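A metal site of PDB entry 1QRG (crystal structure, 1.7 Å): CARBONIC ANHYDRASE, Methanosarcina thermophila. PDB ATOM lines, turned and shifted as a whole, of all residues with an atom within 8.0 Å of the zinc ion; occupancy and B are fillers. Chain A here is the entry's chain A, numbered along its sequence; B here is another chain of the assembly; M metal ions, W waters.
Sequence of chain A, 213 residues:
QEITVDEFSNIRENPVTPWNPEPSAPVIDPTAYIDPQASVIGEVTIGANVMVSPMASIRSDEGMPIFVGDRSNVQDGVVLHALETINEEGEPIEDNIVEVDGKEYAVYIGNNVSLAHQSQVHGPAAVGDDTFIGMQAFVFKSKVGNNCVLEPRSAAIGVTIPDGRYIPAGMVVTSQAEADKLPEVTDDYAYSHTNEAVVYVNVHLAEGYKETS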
ATOM      1  N   ARG A  59       7.760 -23.308   6.613  1.00  0.00           N
ATOM      2  CA  ARG A  59       6.632 -24.190   6.324  1.00  0.00           C
ATOM      3  C   ARG A  59       7.198 -25.561   5.951  1.00  0.00           C
ATOM      4  O   ARG A  59       7.826 -25.692   4.904  1.00  0.00           O
ATOM      5  CB  ARG A  59       5.818 -23.580   5.146  1.00  0.00           C
ATOM      6  CG  ARG A  59       4.578 -24.447   4.788  1.00  0.00           C
ATOM      7  CD  ARG A  59       3.558 -23.564   4.084  1.00  0.00           C
ATOM      8  NE  ARG A  59       4.031 -23.136   2.718  1.00  0.00           N
ATOM      9  CZ  ARG A  59       3.847 -23.770   1.571  1.00  0.00           C
ATOM     10  NH1 ARG A  59       3.186 -24.946   1.514  1.00  0.00           N
ATOM     11  NH2 ARG A  59       4.286 -23.212   0.421  1.00  0.00           N
ATOM     12  N   ASP A  61       5.926 -28.748   5.319  1.00  0.00           N
ATOM     13  CA  ASP A  61       4.715 -29.519   4.990  1.00  0.00           C
ATOM     14  C   ASP A  61       4.899 -30.356   3.729  1.00  0.00           C
ATOM     15  O   ASP A  61       4.042 -31.184   3.365  1.00  0.00           O
ATOM     16  CB  ASP A  61       3.491 -28.615   4.838  1.00  0.00           C
ATOM     17  CG  ASP A  61       3.652 -27.556   3.715  1.00  0.00           C
ATOM     18  OD1 ASP A  61       2.707 -26.736   3.574  1.00  0.00           O
ATOM     19  OD2 ASP A  61       4.691 -27.579   3.052  1.00  0.00           O
ATOM     20  N   GLU A  62       6.038 -30.103   3.035  1.00  0.00           N
ATOM     21  CA  GLU A  62       6.333 -30.829   1.796  1.00  0.00           C
ATOM     22  C   GLU A  62       7.605 -31.615   2.138  1.00  0.00           C
ATOM     23  O   GLU A  62       7.477 -32.716   2.692  1.00  0.00           O
ATOM     24  CB  GLU A  62       6.487 -29.907   0.588  1.00  0.00           C
ATOM     25  CG  GLU A  62       6.752 -30.592  -0.743  1.00  0.00           C
ATOM     26  CD  GLU A  62       6.882 -29.693  -1.953  1.00  0.00           C
ATOM     27  OE1 GLU A  62       6.309 -28.601  -1.849  1.00  0.00           O
ATOM     28  OE2 GLU A  62       7.494 -30.082  -2.997  1.00  0.00           O
ATOM     29  N   GLY A  63       8.752 -31.012   1.887  1.00  0.00           N
ATOM     30  CA  GLY A  63      10.054 -31.533   2.316  1.00  0.00           C
ATOM     31  C   GLY A  63      10.173 -31.287   3.830  1.00  0.00           C
ATOM     32  O   GLY A  63       9.762 -30.224   4.357  1.00  0.00           O
ATOM     33  N   VAL A  79      11.410 -16.821   3.669  1.00  0.00           N
ATOM     34  CA  VAL A  79      10.666 -18.075   3.488  1.00  0.00           C
ATOM     35  C   VAL A  79      11.647 -19.279   3.564  1.00  0.00           C
ATOM     36  O   VAL A  79      12.650 -19.284   2.892  1.00  0.00           O
ATOM     37  CB  VAL A  79       9.928 -18.064   2.153  1.00  0.00           C
ATOM     38  CG1 VAL A  79       9.286 -19.424   1.818  1.00  0.00           C
ATOM     39  CG2 VAL A  79       8.821 -16.978   2.234  1.00  0.00           C
ATOM     40  N   LEU A  80      11.215 -20.278   4.354  1.00  0.00           N
ATOM     41  CA  LEU A  80      11.886 -21.570   4.349  1.00  0.00           C
ATOM     42  C   LEU A  80      10.800 -22.592   3.934  1.00  0.00           C
ATOM     43  O   LEU A  80       9.748 -22.697   4.531  1.00  0.00           O
ATOM     44  CB  LEU A  80      12.391 -21.966   5.768  1.00  0.00           C
ATOM     45  CG  LEU A  80      13.389 -21.000   6.369  1.00  0.00           C
ATOM     46  CD1 LEU A  80      13.812 -21.651   7.747  1.00  0.00           C
ATOM     47  CD2 LEU A  80      14.641 -20.826   5.527  1.00  0.00           C
ATOM     48  N   HIS A  81      11.116 -23.419   2.954  1.00  0.00           N
ATOM     49  CA  HIS A  81      10.208 -24.453   2.447  1.00  0.00           C
ATOM     50  C   HIS A  81      11.067 -25.483   1.710  1.00  0.00           C
ATOM     51  O   HIS A  81      12.274 -25.188   1.483  1.00  0.00           O
ATOM     52  CB  HIS A  81       9.158 -23.862   1.515  1.00  0.00           C
ATOM     53  CG  HIS A  81       8.065 -24.835   1.245  1.00  0.00           C
ATOM     54  ND1 HIS A  81       7.788 -25.390   0.061  1.00  0.00           N
ATOM     55  CD2 HIS A  81       7.104 -25.338   2.047  1.00  0.00           C
ATOM     56  CE1 HIS A  81       6.749 -26.221   0.024  1.00  0.00           C
ATOM     57  NE2 HIS A  81       6.319 -26.212   1.266  1.00  0.00           N
ATOM     58  N   ALA A  82      10.520 -26.653   1.333  1.00  0.00           N
ATOM     59  CA  ALA A  82      11.450 -27.574   0.668  1.00  0.00           C
ATOM     60  C   ALA A  82      10.721 -28.545  -0.270  1.00  0.00           C
ATOM     61  O   ALA A  82       9.523 -28.753  -0.141  1.00  0.00           O
ATOM     62  CB  ALA A  82      12.061 -28.454   1.789  1.00  0.00           C
ATOM     63  N   LEU A  83      11.478 -29.017  -1.257  1.00  0.00           N
ATOM     64  CA  LEU A  83      10.930 -30.042  -2.157  1.00  0.00           C
ATOM     65  C   LEU A  83      10.637 -31.340  -1.451  1.00  0.00           C
ATOM     66  O   LEU A  83      11.205 -31.677  -0.398  1.00  0.00           O
ATOM     67  CB  LEU A  83      11.961 -30.337  -3.280  1.00  0.00           C
ATOM     68  CG  LEU A  83      12.328 -29.144  -4.175  1.00  0.00           C
ATOM     69  CD1 LEU A  83      13.461 -29.560  -5.107  1.00  0.00           C
ATOM     70  CD2 LEU A  83      11.120 -28.697  -4.968  1.00  0.00           C
ATOM     71  N   GLU A  84       9.632 -32.071  -1.947  1.00  0.00           N
ATOM     72  CA  GLU A  84       9.231 -33.309  -1.278  1.00  0.00           C
ATOM     73  C   GLU A  84      10.403 -34.257  -1.044  1.00  0.00           C
ATOM     74  O   GLU A  84      11.370 -34.444  -1.794  1.00  0.00           O
ATOM     75  CB  GLU A  84       8.121 -33.947  -2.144  1.00  0.00           C
ATOM     76  CG  GLU A  84       8.621 -34.229  -3.546  1.00  0.00           C
ATOM     77  CD  GLU A  84       7.981 -33.399  -4.652  1.00  0.00           C
ATOM     78  OE1 GLU A  84       8.319 -32.203  -4.795  1.00  0.00           O
ATOM     79  OE2 GLU A  84       7.159 -33.971  -5.400  1.00  0.00           O
ATOM     80  N   GLN A 120      15.555 -16.220   1.068  1.00  0.00           N
ATOM     81  CA  GLN A 120      14.781 -17.485   1.028  1.00  0.00           C
ATOM     82  C   GLN A 120      15.803 -18.639   0.953  1.00  0.00           C
ATOM     83  O   GLN A 120      16.741 -18.507   0.161  1.00  0.00           O
ATOM     84  CB  GLN A 120      13.893 -17.520  -0.208  1.00  0.00           C
ATOM     85  CG  GLN A 120      13.255 -18.890  -0.489  1.00  0.00           C
ATOM     86  CD  GLN A 120      12.238 -18.900  -1.639  1.00  0.00           C
ATOM     87  OE1 GLN A 120      11.852 -20.039  -2.016  1.00  0.00           O
ATOM     88  NE2 GLN A 120      11.780 -17.785  -2.200  1.00  0.00           N
ATOM     89  N   VAL A 121      15.555 -19.687   1.685  1.00  0.00           N
ATOM     90  CA  VAL A 121      16.389 -20.912   1.596  1.00  0.00           C
ATOM     91  C   VAL A 121      15.402 -22.015   1.315  1.00  0.00           C
ATOM     92  O   VAL A 121      14.480 -22.238   2.116  1.00  0.00           O
ATOM     93  CB  VAL A 121      17.173 -21.169   2.865  1.00  0.00           C
ATOM     94  CG1 VAL A 121      17.984 -22.476   2.621  1.00  0.00           C
ATOM     95  CG2 VAL A 121      18.099 -20.011   3.213  1.00  0.00           C
ATOM     96  N   HIS A 122      15.530 -22.649   0.138  1.00  0.00           N
ATOM     97  CA  HIS A 122      14.575 -23.665  -0.242  1.00  0.00           C
ATOM     98  C   HIS A 122      15.250 -25.030  -0.324  1.00  0.00           C
ATOM     99  O   HIS A 122      16.337 -25.117  -0.961  1.00  0.00           O
ATOM    100  CB  HIS A 122      14.096 -23.243  -1.682  1.00  0.00           C
ATOM    101  CG  HIS A 122      12.842 -24.029  -1.908  1.00  0.00           C
ATOM    102  ND1 HIS A 122      12.814 -25.367  -2.213  1.00  0.00           N
ATOM    103  CD2 HIS A 122      11.576 -23.533  -1.867  1.00  0.00           C
ATOM    104  CE1 HIS A 122      11.582 -25.769  -2.341  1.00  0.00           C
ATOM    105  NE2 HIS A 122      10.875 -24.661  -2.158  1.00  0.00           N
ATOM    106  N   GLY A 123      14.674 -25.987   0.357  1.00  0.00           N
ATOM    107  CA  GLY A 123      15.329 -27.327   0.355  1.00  0.00           C
ATOM    108  C   GLY A 123      15.225 -28.004  -1.010  1.00  0.00           C
ATOM    109  O   GLY A 123      14.340 -27.711  -1.795  1.00  0.00           O
ATOM    110  N   PHE A 140      19.111 -22.558  -2.962  1.00  0.00           N
ATOM    111  CA  PHE A 140      18.242 -23.646  -3.337  1.00  0.00           C
ATOM    112  C   PHE A 140      19.136 -24.792  -3.877  1.00  0.00           C
ATOM    113  O   PHE A 140      20.081 -24.469  -4.621  1.00  0.00           O
ATOM    114  CB  PHE A 140      17.322 -23.110  -4.439  1.00  0.00           C
ATOM    115  CG  PHE A 140      16.441 -24.173  -5.053  1.00  0.00           C
ATOM    116  CD1 PHE A 140      15.788 -25.108  -4.267  1.00  0.00           C
ATOM    117  CD2 PHE A 140      16.228 -24.162  -6.418  1.00  0.00           C
ATOM    118  CE1 PHE A 140      14.927 -26.017  -4.847  1.00  0.00           C
ATOM    119  CE2 PHE A 140      15.339 -25.054  -6.984  1.00  0.00           C
ATOM    120  CZ  PHE A 140      14.701 -25.996  -6.216  1.00  0.00           C
ATOM    121  N   GLN B  75       2.162 -19.219  -3.749  1.00  0.00           N
ATOM    122  CA  GLN B  75       3.021 -19.559  -2.591  1.00  0.00           C
ATOM    123  C   GLN B  75       3.380 -18.370  -1.688  1.00  0.00           C
ATOM    124  O   GLN B  75       2.865 -17.286  -1.789  1.00  0.00           O
ATOM    125  CB  GLN B  75       4.261 -20.362  -2.982  1.00  0.00           C
ATOM    126  CG  GLN B  75       3.794 -21.629  -3.788  1.00  0.00           C
ATOM    127  CD  GLN B  75       5.013 -22.371  -4.293  1.00  0.00           C
ATOM    128  OE1 GLN B  75       6.147 -22.292  -3.799  1.00  0.00           O
ATOM    129  NE2 GLN B  75       4.809 -23.222  -5.298  1.00  0.00           N
ATOM    130  N   ASP B  76       4.163 -18.703  -0.656  1.00  0.00           N
ATOM    131  CA  ASP B  76       4.337 -17.828   0.478  1.00  0.00           C
ATOM    132  C   ASP B  76       4.983 -16.505  -0.034  1.00  0.00           C
ATOM    133  O   ASP B  76       5.920 -16.481  -0.805  1.00  0.00           O
ATOM    134  CB  ASP B  76       5.266 -18.334   1.600  1.00  0.00           C
ATOM    135  CG  ASP B  76       5.080 -19.838   1.860  1.00  0.00           C
ATOM    136  OD1 ASP B  76       5.291 -20.638   0.942  1.00  0.00           O
ATOM    137  OD2 ASP B  76       4.736 -20.191   3.003  1.00  0.00           O
ATOM    138  N   ALA B 116       5.763 -19.578  -7.461  1.00  0.00           N
ATOM    139  CA  ALA B 116       6.547 -20.020  -6.298  1.00  0.00           C
ATOM    140  C   ALA B 116       6.877 -18.920  -5.309  1.00  0.00           C
ATOM    141  O   ALA B 116       6.725 -17.732  -5.553  1.00  0.00           O
ATOM    142  CB  ALA B 116       7.732 -20.840  -6.771  1.00  0.00           C
ATOM    143  N   HIS B 117       7.416 -19.340  -4.177  1.00  0.00           N
ATOM    144  CA  HIS B 117       7.665 -18.423  -3.056  1.00  0.00           C
ATOM    145  C   HIS B 117       8.274 -17.088  -3.373  1.00  0.00           C
ATOM    146  O   HIS B 117       9.352 -17.099  -4.029  1.00  0.00           O
ATOM    147  CB  HIS B 117       8.546 -19.058  -1.985  1.00  0.00           C
ATOM    148  CG  HIS B 117       8.300 -20.519  -1.764  1.00  0.00           C
ATOM    149  ND1 HIS B 117       7.269 -20.917  -0.933  1.00  0.00           N
ATOM    150  CD2 HIS B 117       8.934 -21.608  -2.249  1.00  0.00           C
ATOM    151  CE1 HIS B 117       7.231 -22.221  -0.858  1.00  0.00           C
ATOM    152  NE2 HIS B 117       8.182 -22.605  -1.708  1.00  0.00           N
ATOM    153  N   PHE B 132       5.522 -22.710 -14.640  1.00  0.00           N
ATOM    154  CA  PHE B 132       6.129 -22.529 -13.322  1.00  0.00           C
ATOM    155  C   PHE B 132       6.737 -21.140 -13.283  1.00  0.00           C
ATOM    156  O   PHE B 132       7.695 -20.833 -14.015  1.00  0.00           O
ATOM    157  CB  PHE B 132       7.161 -23.643 -13.087  1.00  0.00           C
ATOM    158  CG  PHE B 132       7.923 -23.579 -11.786  1.00  0.00           C
ATOM    159  CD1 PHE B 132       7.356 -24.104 -10.631  1.00  0.00           C
ATOM    160  CD2 PHE B 132       9.159 -22.986 -11.720  1.00  0.00           C
ATOM    161  CE1 PHE B 132       8.087 -24.048  -9.444  1.00  0.00           C
ATOM    162  CE2 PHE B 132       9.905 -22.931 -10.559  1.00  0.00           C
ATOM    163  CZ  PHE B 132       9.341 -23.449  -9.374  1.00  0.00           C
ATOM    164  N   MET B 135      10.901 -19.175  -7.796  1.00  0.00           N
ATOM    165  CA  MET B 135      11.076 -18.391  -6.555  1.00  0.00           C
ATOM    166  C   MET B 135      11.695 -17.032  -6.845  1.00  0.00           C
ATOM    167  O   MET B 135      12.666 -16.921  -7.605  1.00  0.00           O
ATOM    168  CB  MET B 135      11.954 -19.190  -5.601  1.00  0.00           C
ATOM    169  CG  MET B 135      11.522 -20.579  -5.159  1.00  0.00           C
ATOM    170  SD  MET B 135      11.931 -21.863  -6.356  1.00  0.00           S
ATOM    171  CE  MET B 135      11.222 -23.333  -5.626  1.00  0.00           C
ATOM    172  N   VAL B 198       4.903 -29.796  -8.602  1.00  0.00           N
ATOM    173  CA  VAL B 198       4.483 -28.771  -7.685  1.00  0.00           C
ATOM    174  C   VAL B 198       2.936 -28.746  -7.617  1.00  0.00           C
ATOM    175  O   VAL B 198       2.325 -28.472  -6.557  1.00  0.00           O
ATOM    176  CB  VAL B 198       5.047 -27.397  -8.119  1.00  0.00           C
ATOM    177  CG1 VAL B 198       4.691 -26.294  -7.163  1.00  0.00           C
ATOM    178  CG2 VAL B 198       6.584 -27.600  -8.238  1.00  0.00           C
ATOM    179  N   VAL B 201       1.581 -31.717  -5.716  1.00  0.00           N
ATOM    180  CA  VAL B 201       1.791 -31.447  -4.288  1.00  0.00           C
ATOM    181  C   VAL B 201       0.822 -30.423  -3.769  1.00  0.00           C
ATOM    182  O   VAL B 201       0.274 -30.604  -2.678  1.00  0.00           O
ATOM    183  CB  VAL B 201       3.251 -30.951  -4.045  1.00  0.00           C
ATOM    184  CG1 VAL B 201       3.446 -30.336  -2.667  1.00  0.00           C
ATOM    185  CG2 VAL B 201       4.161 -32.139  -4.284  1.00  0.00           C
ATOM    186  N   ASN B 202       0.688 -29.255  -4.408  1.00  0.00           N
ATOM    187  CA  ASN B 202      -0.132 -28.186  -3.915  1.00  0.00           C
ATOM    188  C   ASN B 202      -1.610 -28.499  -3.881  1.00  0.00           C
ATOM    189  O   ASN B 202      -2.356 -28.068  -3.009  1.00  0.00           O
ATOM    190  CB  ASN B 202       0.124 -26.813  -4.603  1.00  0.00           C
ATOM    191  CG  ASN B 202       1.378 -26.136  -3.975  1.00  0.00           C
ATOM    192  OD1 ASN B 202       1.219 -25.358  -3.014  1.00  0.00           O
ATOM    193  ND2 ASN B 202       2.517 -26.457  -4.547  1.00  0.00           N
ATOM    194  N   LEU B 205      -1.851 -30.511  -0.779  1.00  0.00           N
ATOM    195  CA  LEU B 205      -1.761 -29.628   0.402  1.00  0.00           C
ATOM    196  C   LEU B 205      -3.036 -28.861   0.623  1.00  0.00           C
ATOM    197  O   LEU B 205      -3.482 -28.682   1.766  1.00  0.00           O
ATOM    198  CB  LEU B 205      -0.605 -28.611   0.270  1.00  0.00           C
ATOM    199  CG  LEU B 205       0.786 -29.168   0.424  1.00  0.00           C
ATOM    200  CD1 LEU B 205       1.826 -28.101   0.065  1.00  0.00           C
ATOM    201  CD2 LEU B 205       1.021 -29.583   1.907  1.00  0.00           C
HETATM  202 ZN    ZN M   1       8.648 -24.729  -1.971  1.00  0.00          ZN
HETATM  203  O   HOH W   1       7.515 -24.831  -3.657  1.00  0.00           O
HETATM  204  O   HOH W   2       8.558 -26.754  -2.719  1.00  0.00           O
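The side-chain amide oxygen (OE1) of Gln 75 of chain B sits close to the backbone NH (N) of His 117 of chain B, at 3.2 Å.
The backbone carbonyl oxygen (O) of His 117 of chain B lies within hydrogen-bond range of the side-chain amide nitrogen (NE2) of Gln 120, 3.1 Å away.
ND1 of His 117 of chain B sits at hydrogen-bond distance from OD1 of Asp 76 of chain B, at 2.7 Å.
The guanidinium group (NH1) of Arg 59 is in hydrogen-bond range of a ring nitrogen (NE2) of His 81 (3.4 Å).
The backbone carbonyl oxygen (O) of His 81 lies within hydrogen-bond range of the backbone NH (N) of Gly 123.
NE2 of His 81 lies within hydrogen-bond range of OD2 of Asp 61, at 2.8 Å.
Gln 75 of chain B touches the zinc ion.
Four residues have an atom within 4 Å of the zinc ion: His 81, His 122, Gln 75 of chain B and His 117 of chain B.
Water W2 lies within hydrogen-bond range of OE1 of Glu 62 (3.0 Å) and O of Ala 82 (3.4 Å).
The zinc ion is bound by water W1 (2.0 Å), water W2 (2.2 Å), a ring nitrogen (NE2) of His 117 of chain B (2.2 Å), a ring nitrogen (NE2) of His 122 (2.2 Å) and a ring nitrogen (ND1) of His 81 (2.3 Å).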
